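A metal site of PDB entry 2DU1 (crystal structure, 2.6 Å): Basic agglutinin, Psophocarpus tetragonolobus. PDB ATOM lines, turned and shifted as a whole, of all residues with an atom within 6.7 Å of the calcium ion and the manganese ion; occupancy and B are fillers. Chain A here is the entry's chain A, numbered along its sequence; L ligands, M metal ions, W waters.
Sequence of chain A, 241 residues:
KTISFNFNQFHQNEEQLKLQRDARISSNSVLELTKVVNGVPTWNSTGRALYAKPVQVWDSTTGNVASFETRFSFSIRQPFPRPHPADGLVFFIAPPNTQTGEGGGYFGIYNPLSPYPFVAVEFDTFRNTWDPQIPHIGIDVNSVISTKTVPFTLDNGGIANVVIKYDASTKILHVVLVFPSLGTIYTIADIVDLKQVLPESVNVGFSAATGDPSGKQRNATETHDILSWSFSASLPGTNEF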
ATOM      1  N   ASP A  87     -10.699  -2.566  22.069  1.00  0.00           N
ATOM      2  CA  ASP A  87     -11.781  -2.432  23.036  1.00  0.00           C
ATOM      3  C   ASP A  87     -12.683  -3.666  23.064  1.00  0.00           C
ATOM      4  O   ASP A  87     -13.372  -3.927  24.058  1.00  0.00           O
ATOM      5  CB  ASP A  87     -12.624  -1.191  22.712  1.00  0.00           C
ATOM      6  CG  ASP A  87     -12.098   0.055  23.382  1.00  0.00           C
ATOM      7  OD1 ASP A  87     -11.195   0.709  22.791  1.00  0.00           O
ATOM      8  OD2 ASP A  87     -12.570   0.382  24.492  1.00  0.00           O
ATOM      9  N   GLY A 104     -13.733   3.390  20.324  1.00  0.00           N
ATOM     10  CA  GLY A 104     -13.497   3.113  21.736  1.00  0.00           C
ATOM     11  C   GLY A 104     -14.532   2.185  22.355  1.00  0.00           C
ATOM     12  O   GLY A 104     -14.968   1.218  21.717  1.00  0.00           O
ATOM     13  N   GLY A 105     -14.920   2.475  23.590  1.00  0.00           N
ATOM     14  CA  GLY A 105     -15.883   1.658  24.288  1.00  0.00           C
ATOM     15  C   GLY A 105     -17.245   1.560  23.650  1.00  0.00           C
ATOM     16  O   GLY A 105     -18.081   0.797  24.123  1.00  0.00           O
ATOM     17  N   TYR A 106     -17.476   2.316  22.578  1.00  0.00           N
ATOM     18  CA  TYR A 106     -18.779   2.253  21.893  1.00  0.00           C
ATOM     19  C   TYR A 106     -18.764   1.290  20.717  1.00  0.00           C
ATOM     20  O   TYR A 106     -19.765   1.115  20.034  1.00  0.00           O
ATOM     21  CB  TYR A 106     -19.219   3.641  21.439  1.00  0.00           C
ATOM     22  CG  TYR A 106     -19.478   4.583  22.589  1.00  0.00           C
ATOM     23  CD1 TYR A 106     -20.530   4.370  23.472  1.00  0.00           C
ATOM     24  CD2 TYR A 106     -18.632   5.662  22.816  1.00  0.00           C
ATOM     25  CE1 TYR A 106     -20.725   5.207  24.576  1.00  0.00           C
ATOM     26  CE2 TYR A 106     -18.823   6.509  23.910  1.00  0.00           C
ATOM     27  CZ  TYR A 106     -19.873   6.276  24.784  1.00  0.00           C
ATOM     28  OH  TYR A 106     -20.042   7.111  25.876  1.00  0.00           O
ATOM     29  N   PHE A 107     -17.610   0.670  20.491  1.00  0.00           N
ATOM     30  CA  PHE A 107     -17.464  -0.351  19.456  1.00  0.00           C
ATOM     31  C   PHE A 107     -17.789   0.079  18.037  1.00  0.00           C
ATOM     32  O   PHE A 107     -17.716  -0.733  17.112  1.00  0.00           O
ATOM     33  CB  PHE A 107     -18.347  -1.550  19.816  1.00  0.00           C
ATOM     34  CG  PHE A 107     -18.180  -2.044  21.230  1.00  0.00           C
ATOM     35  CD1 PHE A 107     -17.011  -2.682  21.632  1.00  0.00           C
ATOM     36  CD2 PHE A 107     -19.208  -1.904  22.161  1.00  0.00           C
ATOM     37  CE1 PHE A 107     -16.864  -3.192  22.946  1.00  0.00           C
ATOM     38  CE2 PHE A 107     -19.080  -2.413  23.469  1.00  0.00           C
ATOM     39  CZ  PHE A 107     -17.917  -3.052  23.858  1.00  0.00           C
ATOM     40  N   GLU A 122     -21.848  -8.289  22.980  1.00  0.00           N
ATOM     41  CA  GLU A 122     -20.477  -7.820  23.038  1.00  0.00           C
ATOM     42  C   GLU A 122     -19.493  -8.757  23.725  1.00  0.00           C
ATOM     43  O   GLU A 122     -19.860  -9.549  24.595  1.00  0.00           O
ATOM     44  CB  GLU A 122     -20.412  -6.472  23.772  1.00  0.00           C
ATOM     45  CG  GLU A 122     -20.714  -6.603  25.263  1.00  0.00           C
ATOM     46  CD  GLU A 122     -20.559  -5.297  26.040  1.00  0.00           C
ATOM     47  OE1 GLU A 122     -21.130  -4.273  25.609  1.00  0.00           O
ATOM     48  OE2 GLU A 122     -19.892  -5.309  27.091  1.00  0.00           O
ATOM     49  N   ASP A 124     -16.435  -7.632  25.397  1.00  0.00           N
ATOM     50  CA  ASP A 124     -15.755  -6.461  25.912  1.00  0.00           C
ATOM     51  C   ASP A 124     -14.427  -6.792  26.556  1.00  0.00           C
ATOM     52  O   ASP A 124     -14.373  -7.598  27.490  1.00  0.00           O
ATOM     53  CB  ASP A 124     -16.669  -5.808  26.952  1.00  0.00           C
ATOM     54  CG  ASP A 124     -16.402  -4.318  27.110  1.00  0.00           C
ATOM     55  OD1 ASP A 124     -15.233  -3.901  27.170  1.00  0.00           O
ATOM     56  OD2 ASP A 124     -17.390  -3.572  27.193  1.00  0.00           O
ATOM     57  N   THR A 125     -13.355  -6.148  26.094  1.00  0.00           N
ATOM     58  CA  THR A 125     -12.021  -6.405  26.630  1.00  0.00           C
ATOM     59  C   THR A 125     -11.428  -5.244  27.443  1.00  0.00           C
ATOM     60  O   THR A 125     -10.419  -5.401  28.109  1.00  0.00           O
ATOM     61  CB  THR A 125     -11.045  -6.794  25.487  1.00  0.00           C
ATOM     62  OG1 THR A 125     -11.103  -5.835  24.416  1.00  0.00           O
ATOM     63  CG2 THR A 125     -11.408  -8.180  24.953  1.00  0.00           C
ATOM     64  N   PHE A 126     -12.080  -4.078  27.397  1.00  0.00           N
ATOM     65  CA  PHE A 126     -11.614  -2.915  28.148  1.00  0.00           C
ATOM     66  C   PHE A 126     -12.673  -2.461  29.133  1.00  0.00           C
ATOM     67  O   PHE A 126     -13.850  -2.331  28.783  1.00  0.00           O
ATOM     68  CB  PHE A 126     -11.318  -1.754  27.200  1.00  0.00           C
ATOM     69  CG  PHE A 126     -10.838  -0.534  27.909  1.00  0.00           C
ATOM     70  CD1 PHE A 126      -9.498  -0.410  28.264  1.00  0.00           C
ATOM     71  CD2 PHE A 126     -11.732   0.473  28.269  1.00  0.00           C
ATOM     72  CE1 PHE A 126      -9.050   0.721  28.969  1.00  0.00           C
ATOM     73  CE2 PHE A 126     -11.303   1.594  28.968  1.00  0.00           C
ATOM     74  CZ  PHE A 126      -9.963   1.718  29.323  1.00  0.00           C
ATOM     75  N   ARG A 127     -12.257  -2.184  30.357  1.00  0.00           N
ATOM     76  CA  ARG A 127     -13.203  -1.751  31.380  1.00  0.00           C
ATOM     77  C   ARG A 127     -13.468  -0.257  31.396  1.00  0.00           C
ATOM     78  O   ARG A 127     -12.652   0.517  31.886  1.00  0.00           O
ATOM     79  CB  ARG A 127     -12.731  -2.200  32.764  1.00  0.00           C
ATOM     80  CG  ARG A 127     -13.772  -1.942  33.841  1.00  0.00           C
ATOM     81  CD  ARG A 127     -13.458  -2.638  35.148  1.00  0.00           C
ATOM     82  NE  ARG A 127     -14.637  -2.606  36.016  1.00  0.00           N
ATOM     83  CZ  ARG A 127     -14.668  -3.061  37.268  1.00  0.00           C
ATOM     84  NH1 ARG A 127     -13.576  -3.578  37.816  1.00  0.00           N
ATOM     85  NH2 ARG A 127     -15.801  -2.998  37.969  1.00  0.00           N
ATOM     86  N   ASN A 128     -14.622   0.154  30.867  1.00  0.00           N
ATOM     87  CA  ASN A 128     -15.004   1.563  30.883  1.00  0.00           C
ATOM     88  C   ASN A 128     -15.667   1.830  32.220  1.00  0.00           C
ATOM     89  O   ASN A 128     -15.900   0.907  32.994  1.00  0.00           O
ATOM     90  CB  ASN A 128     -15.978   1.874  29.734  1.00  0.00           C
ATOM     91  CG  ASN A 128     -15.338   1.887  28.361  1.00  0.00           C
ATOM     92  OD1 ASN A 128     -15.308   0.858  27.679  1.00  0.00           O
ATOM     93  ND2 ASN A 128     -14.838   3.038  27.943  1.00  0.00           N
ATOM     94  N   TRP A 130     -18.590   2.327  32.952  1.00  0.00           N
ATOM     95  CA  TRP A 130     -19.862   1.623  33.057  1.00  0.00           C
ATOM     96  C   TRP A 130     -19.747   0.101  32.983  1.00  0.00           C
ATOM     97  O   TRP A 130     -20.763  -0.591  32.950  1.00  0.00           O
ATOM     98  CB  TRP A 130     -20.791   2.094  31.944  1.00  0.00           C
ATOM     99  CG  TRP A 130     -20.230   1.801  30.597  1.00  0.00           C
ATOM    100  CD1 TRP A 130     -20.128   0.573  30.004  1.00  0.00           C
ATOM    101  CD2 TRP A 130     -19.608   2.731  29.696  1.00  0.00           C
ATOM    102  NE1 TRP A 130     -19.488   0.675  28.794  1.00  0.00           N
ATOM    103  CE2 TRP A 130     -19.156   1.994  28.584  1.00  0.00           C
ATOM    104  CE3 TRP A 130     -19.396   4.117  29.728  1.00  0.00           C
ATOM    105  CZ2 TRP A 130     -18.501   2.592  27.495  1.00  0.00           C
ATOM    106  CZ3 TRP A 130     -18.744   4.716  28.647  1.00  0.00           C
ATOM    107  CH2 TRP A 130     -18.308   3.960  27.553  1.00  0.00           C
ATOM    108  N   ASP A 131     -18.508  -0.412  32.956  1.00  0.00           N
ATOM    109  CA  ASP A 131     -18.258  -1.850  32.858  1.00  0.00           C
ATOM    110  C   ASP A 131     -17.866  -2.573  34.118  1.00  0.00           C
ATOM    111  O   ASP A 131     -17.265  -1.989  35.024  1.00  0.00           O
ATOM    112  CB  ASP A 131     -17.104  -2.168  31.884  1.00  0.00           C
ATOM    113  CG  ASP A 131     -17.520  -1.954  30.470  1.00  0.00           C
ATOM    114  OD1 ASP A 131     -18.730  -2.101  30.170  1.00  0.00           O
ATOM    115  OD2 ASP A 131     -16.621  -1.683  29.639  1.00  0.00           O
ATOM    116  N   PRO A 132     -18.194  -3.868  34.190  1.00  0.00           N
ATOM    117  CA  PRO A 132     -17.843  -4.705  35.339  1.00  0.00           C
ATOM    118  C   PRO A 132     -16.481  -5.244  34.901  1.00  0.00           C
ATOM    119  O   PRO A 132     -15.979  -4.848  33.848  1.00  0.00           O
ATOM    120  CB  PRO A 132     -18.940  -5.763  35.334  1.00  0.00           C
ATOM    121  CG  PRO A 132     -19.264  -5.914  33.900  1.00  0.00           C
ATOM    122  CD  PRO A 132     -19.293  -4.475  33.418  1.00  0.00           C
ATOM    123  N   ILE A 134     -13.421  -7.150  33.198  1.00  0.00           N
ATOM    124  CA  ILE A 134     -13.293  -7.647  31.839  1.00  0.00           C
ATOM    125  C   ILE A 134     -12.287  -8.801  31.831  1.00  0.00           C
ATOM    126  O   ILE A 134     -11.513  -8.954  32.768  1.00  0.00           O
ATOM    127  CB  ILE A 134     -12.819  -6.534  30.857  1.00  0.00           C
ATOM    128  CG1 ILE A 134     -11.578  -5.815  31.394  1.00  0.00           C
ATOM    129  CG2 ILE A 134     -13.938  -5.549  30.618  1.00  0.00           C
ATOM    130  CD1 ILE A 134     -10.257  -6.524  31.133  1.00  0.00           C
ATOM    131  N   HIS A 136     -15.664  -9.683  29.354  1.00  0.00           N
ATOM    132  CA  HIS A 136     -16.996 -10.165  29.657  1.00  0.00           C
ATOM    133  C   HIS A 136     -17.878 -10.162  28.432  1.00  0.00           C
ATOM    134  O   HIS A 136     -17.624  -9.462  27.447  1.00  0.00           O
ATOM    135  CB  HIS A 136     -17.650  -9.348  30.782  1.00  0.00           C
ATOM    136  CG  HIS A 136     -17.762  -7.874  30.523  1.00  0.00           C
ATOM    137  ND1 HIS A 136     -16.937  -6.955  31.123  1.00  0.00           N
ATOM    138  CD2 HIS A 136     -18.601  -7.169  29.730  1.00  0.00           C
ATOM    139  CE1 HIS A 136     -17.262  -5.739  30.727  1.00  0.00           C
ATOM    140  NE2 HIS A 136     -18.271  -5.842  29.878  1.00  0.00           N
ATOM    141  N   ILE A 137     -18.915 -10.989  28.485  1.00  0.00           N
ATOM    142  CA  ILE A 137     -19.905 -11.074  27.419  1.00  0.00           C
ATOM    143  C   ILE A 137     -21.039 -10.229  27.954  1.00  0.00           C
ATOM    144  O   ILE A 137     -21.336 -10.285  29.146  1.00  0.00           O
ATOM    145  CB  ILE A 137     -20.439 -12.505  27.243  1.00  0.00           C
ATOM    146  CG1 ILE A 137     -19.278 -13.493  27.064  1.00  0.00           C
ATOM    147  CG2 ILE A 137     -21.359 -12.559  26.062  1.00  0.00           C
ATOM    148  CD1 ILE A 137     -19.720 -14.937  27.088  1.00  0.00           C
ATOM    149  N   GLY A 138     -21.654  -9.457  27.092  1.00  0.00           N
ATOM    150  CA  GLY A 138     -22.748  -8.628  27.535  1.00  0.00           C
ATOM    151  C   GLY A 138     -23.832  -8.538  26.480  1.00  0.00           C
ATOM    152  O   GLY A 138     -23.548  -8.642  25.283  1.00  0.00           O
ATOM    153  N   ASP A 140     -26.466  -6.064  24.965  1.00  0.00           N
ATOM    154  CA  ASP A 140     -26.782  -4.651  24.907  1.00  0.00           C
ATOM    155  C   ASP A 140     -28.007  -4.324  24.076  1.00  0.00           C
ATOM    156  O   ASP A 140     -28.168  -4.796  22.958  1.00  0.00           O
ATOM    157  CB  ASP A 140     -25.576  -3.887  24.366  1.00  0.00           C
ATOM    158  CG  ASP A 140     -24.276  -4.222  25.096  1.00  0.00           C
ATOM    159  OD1 ASP A 140     -24.340  -4.609  26.291  1.00  0.00           O
ATOM    160  OD2 ASP A 140     -23.198  -4.098  24.480  1.00  0.00           O
ATOM    161  N   VAL A 144     -24.553   0.586  25.420  1.00  0.00           N
ATOM    162  CA  VAL A 144     -23.406  -0.260  25.649  1.00  0.00           C
ATOM    163  C   VAL A 144     -23.345  -0.586  27.144  1.00  0.00           C
ATOM    164  O   VAL A 144     -22.375  -1.151  27.645  1.00  0.00           O
ATOM    165  CB  VAL A 144     -22.122   0.455  25.188  1.00  0.00           C
ATOM    166  CG1 VAL A 144     -21.911   1.731  25.986  1.00  0.00           C
ATOM    167  CG2 VAL A 144     -20.947  -0.469  25.294  1.00  0.00           C
ATOM    168  N   ILE A 145     -24.402  -0.196  27.860  1.00  0.00           N
ATOM    169  CA  ILE A 145     -24.508  -0.488  29.288  1.00  0.00           C
ATOM    170  C   ILE A 145     -25.354  -1.754  29.337  1.00  0.00           C
ATOM    171  O   ILE A 145     -26.573  -1.698  29.463  1.00  0.00           O
ATOM    172  CB  ILE A 145     -25.212   0.631  30.039  1.00  0.00           C
ATOM    173  CG1 ILE A 145     -24.375   1.906  29.955  1.00  0.00           C
ATOM    174  CG2 ILE A 145     -25.430   0.234  31.480  1.00  0.00           C
ATOM    175  CD1 ILE A 145     -24.935   3.062  30.751  1.00  0.00           C
ATOM    176  N   SER A 146     -24.683  -2.891  29.197  1.00  0.00           N
ATOM    177  CA  SER A 146     -25.322  -4.210  29.159  1.00  0.00           C
ATOM    178  C   SER A 146     -26.419  -4.453  30.177  1.00  0.00           C
ATOM    179  O   SER A 146     -26.342  -4.016  31.322  1.00  0.00           O
ATOM    180  CB  SER A 146     -24.258  -5.296  29.334  1.00  0.00           C
ATOM    181  OG  SER A 146     -23.241  -5.158  28.360  1.00  0.00           O
ATOM    182  N   THR A 149     -24.466  -9.390  31.988  1.00  0.00           N
ATOM    183  CA  THR A 149     -23.048  -9.580  31.756  1.00  0.00           C
ATOM    184  C   THR A 149     -22.522 -10.870  32.402  1.00  0.00           C
ATOM    185  O   THR A 149     -23.044 -11.318  33.420  1.00  0.00           O
ATOM    186  CB  THR A 149     -22.286  -8.356  32.378  1.00  0.00           C
ATOM    187  OG1 THR A 149     -22.060  -7.365  31.376  1.00  0.00           O
ATOM    188  CG2 THR A 149     -20.990  -8.776  33.018  1.00  0.00           C
HETATM  189  O1  LIG L   1      -6.772   3.889  26.323  1.00  0.00           O
HETATM  190  C1  LIG L   1      -7.844   3.123  25.781  1.00  0.00           C
HETATM  191  C2  LIG L   1      -9.190   3.662  26.235  1.00  0.00           C
HETATM  192  O2  LIG L   1      -9.303   5.058  25.812  1.00  0.00           O
HETATM  193  C3  LIG L   1     -10.571   5.712  26.231  1.00  0.00           C
HETATM  194  O3  LIG L   1     -10.729   5.872  27.655  1.00  0.00           O
HETATM  195  C4  LIG L   1      -9.715   6.590  28.371  1.00  0.00           C
HETATM  196  C5  LIG L   1     -11.768   4.919  25.650  1.00  0.00           C
HETATM  197  N1  LIG L   1     -13.019   5.553  26.075  1.00  0.00           N
HETATM  198  C6  LIG L   1     -14.002   5.829  25.210  1.00  0.00           C
HETATM  199  O4  LIG L   1     -13.962   5.574  24.007  1.00  0.00           O
HETATM  200  C7  LIG L   1     -15.255   6.481  25.802  1.00  0.00           C
HETATM  201  C8  LIG L   1     -11.696   3.447  26.127  1.00  0.00           C
HETATM  202  O5  LIG L   1     -12.799   2.704  25.616  1.00  0.00           O
HETATM  203  C9  LIG L   1     -10.366   2.828  25.652  1.00  0.00           C
HETATM  204  O6  LIG L   1     -10.317   2.811  24.215  1.00  0.00           O
HETATM  205 CA    CA M   1     -15.693  -1.628  27.357  1.00  0.00          CA
HETATM  206 MN    MN M   2     -19.048  -3.983  28.787  1.00  0.00          MN
HETATM  207  O   HOH W   1     -19.865  -2.339  27.381  1.00  0.00           O
HETATM  208  O   HOH W   2     -17.710  -0.693  26.417  1.00  0.00           O
HETATM  209  O   HOH W   3     -21.258  -4.011  29.617  1.00  0.00           O
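The side-chain amide nitrogen of Asn 128 sits at hydrogen-bond distance from an oxygen (O5) of the ligand, 3.1 Å away. N of Gly 105 is in hydrogen-bond range of O5 of the ligand (2.9 Å). O5 of the ligand is in hydrogen-bond range of OD2 of Asp 87 (2.6 Å).
N of Glu 122 lies within hydrogen-bond range of O of Gly 138. The guanidinium group (NE) of Arg 127 is in hydrogen-bond range of the backbone carbonyl oxygen (O) of Asp 131, at 2.9 Å. OD1 of Asp 131 lies close to NE1 of Trp 130, 3.2 Å away.
The nearest printed residue that does not touch the calcium ion is Phe 107 (4.4 Å).
Within 4 Å of the manganese ion: Glu 122, Asp 124, Asp 131 and His 136.
The side-chain carboxylate (OD1) of Asp 124 is bound to the calcium ion. Water W2 is bound to the calcium ion (2.4 Å). O of Phe 126 binds the calcium ion. OD2 of Asp 131 binds the calcium ion, at 2.5 Å. OD1 of Asn 128 is bound to the calcium ion (2.5 Å). The calcium ion is bound by OD2 of Asp 124 (2.6 Å). The calcium ion has six donor atoms within binding distance.
The manganese ion is bound by a ring nitrogen (NE2) of His 136 (2.3 Å), water W1 (2.3 Å), the side-chain carboxylate (OE2) of Glu 122 (2.3 Å), the side-chain carboxylate (OD2) of Asp 124 (2.3 Å), the side-chain carboxylate (OD1) of Asp 131 (2.4 Å) and water W3 (2.4 Å). The manganese ion has six donor atoms within binding distance.
Water W2 lies within hydrogen-bond range of the backbone carbonyl oxygen (O) of Gly 105 and the indole nitrogen (NE1) of Trp 130. Water W1 lies within hydrogen-bond range of O of Val 144 (2.8 Å), OE1 of Glu 122 (2.9 Å) and NE1 of Trp 130 (3.4 Å).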
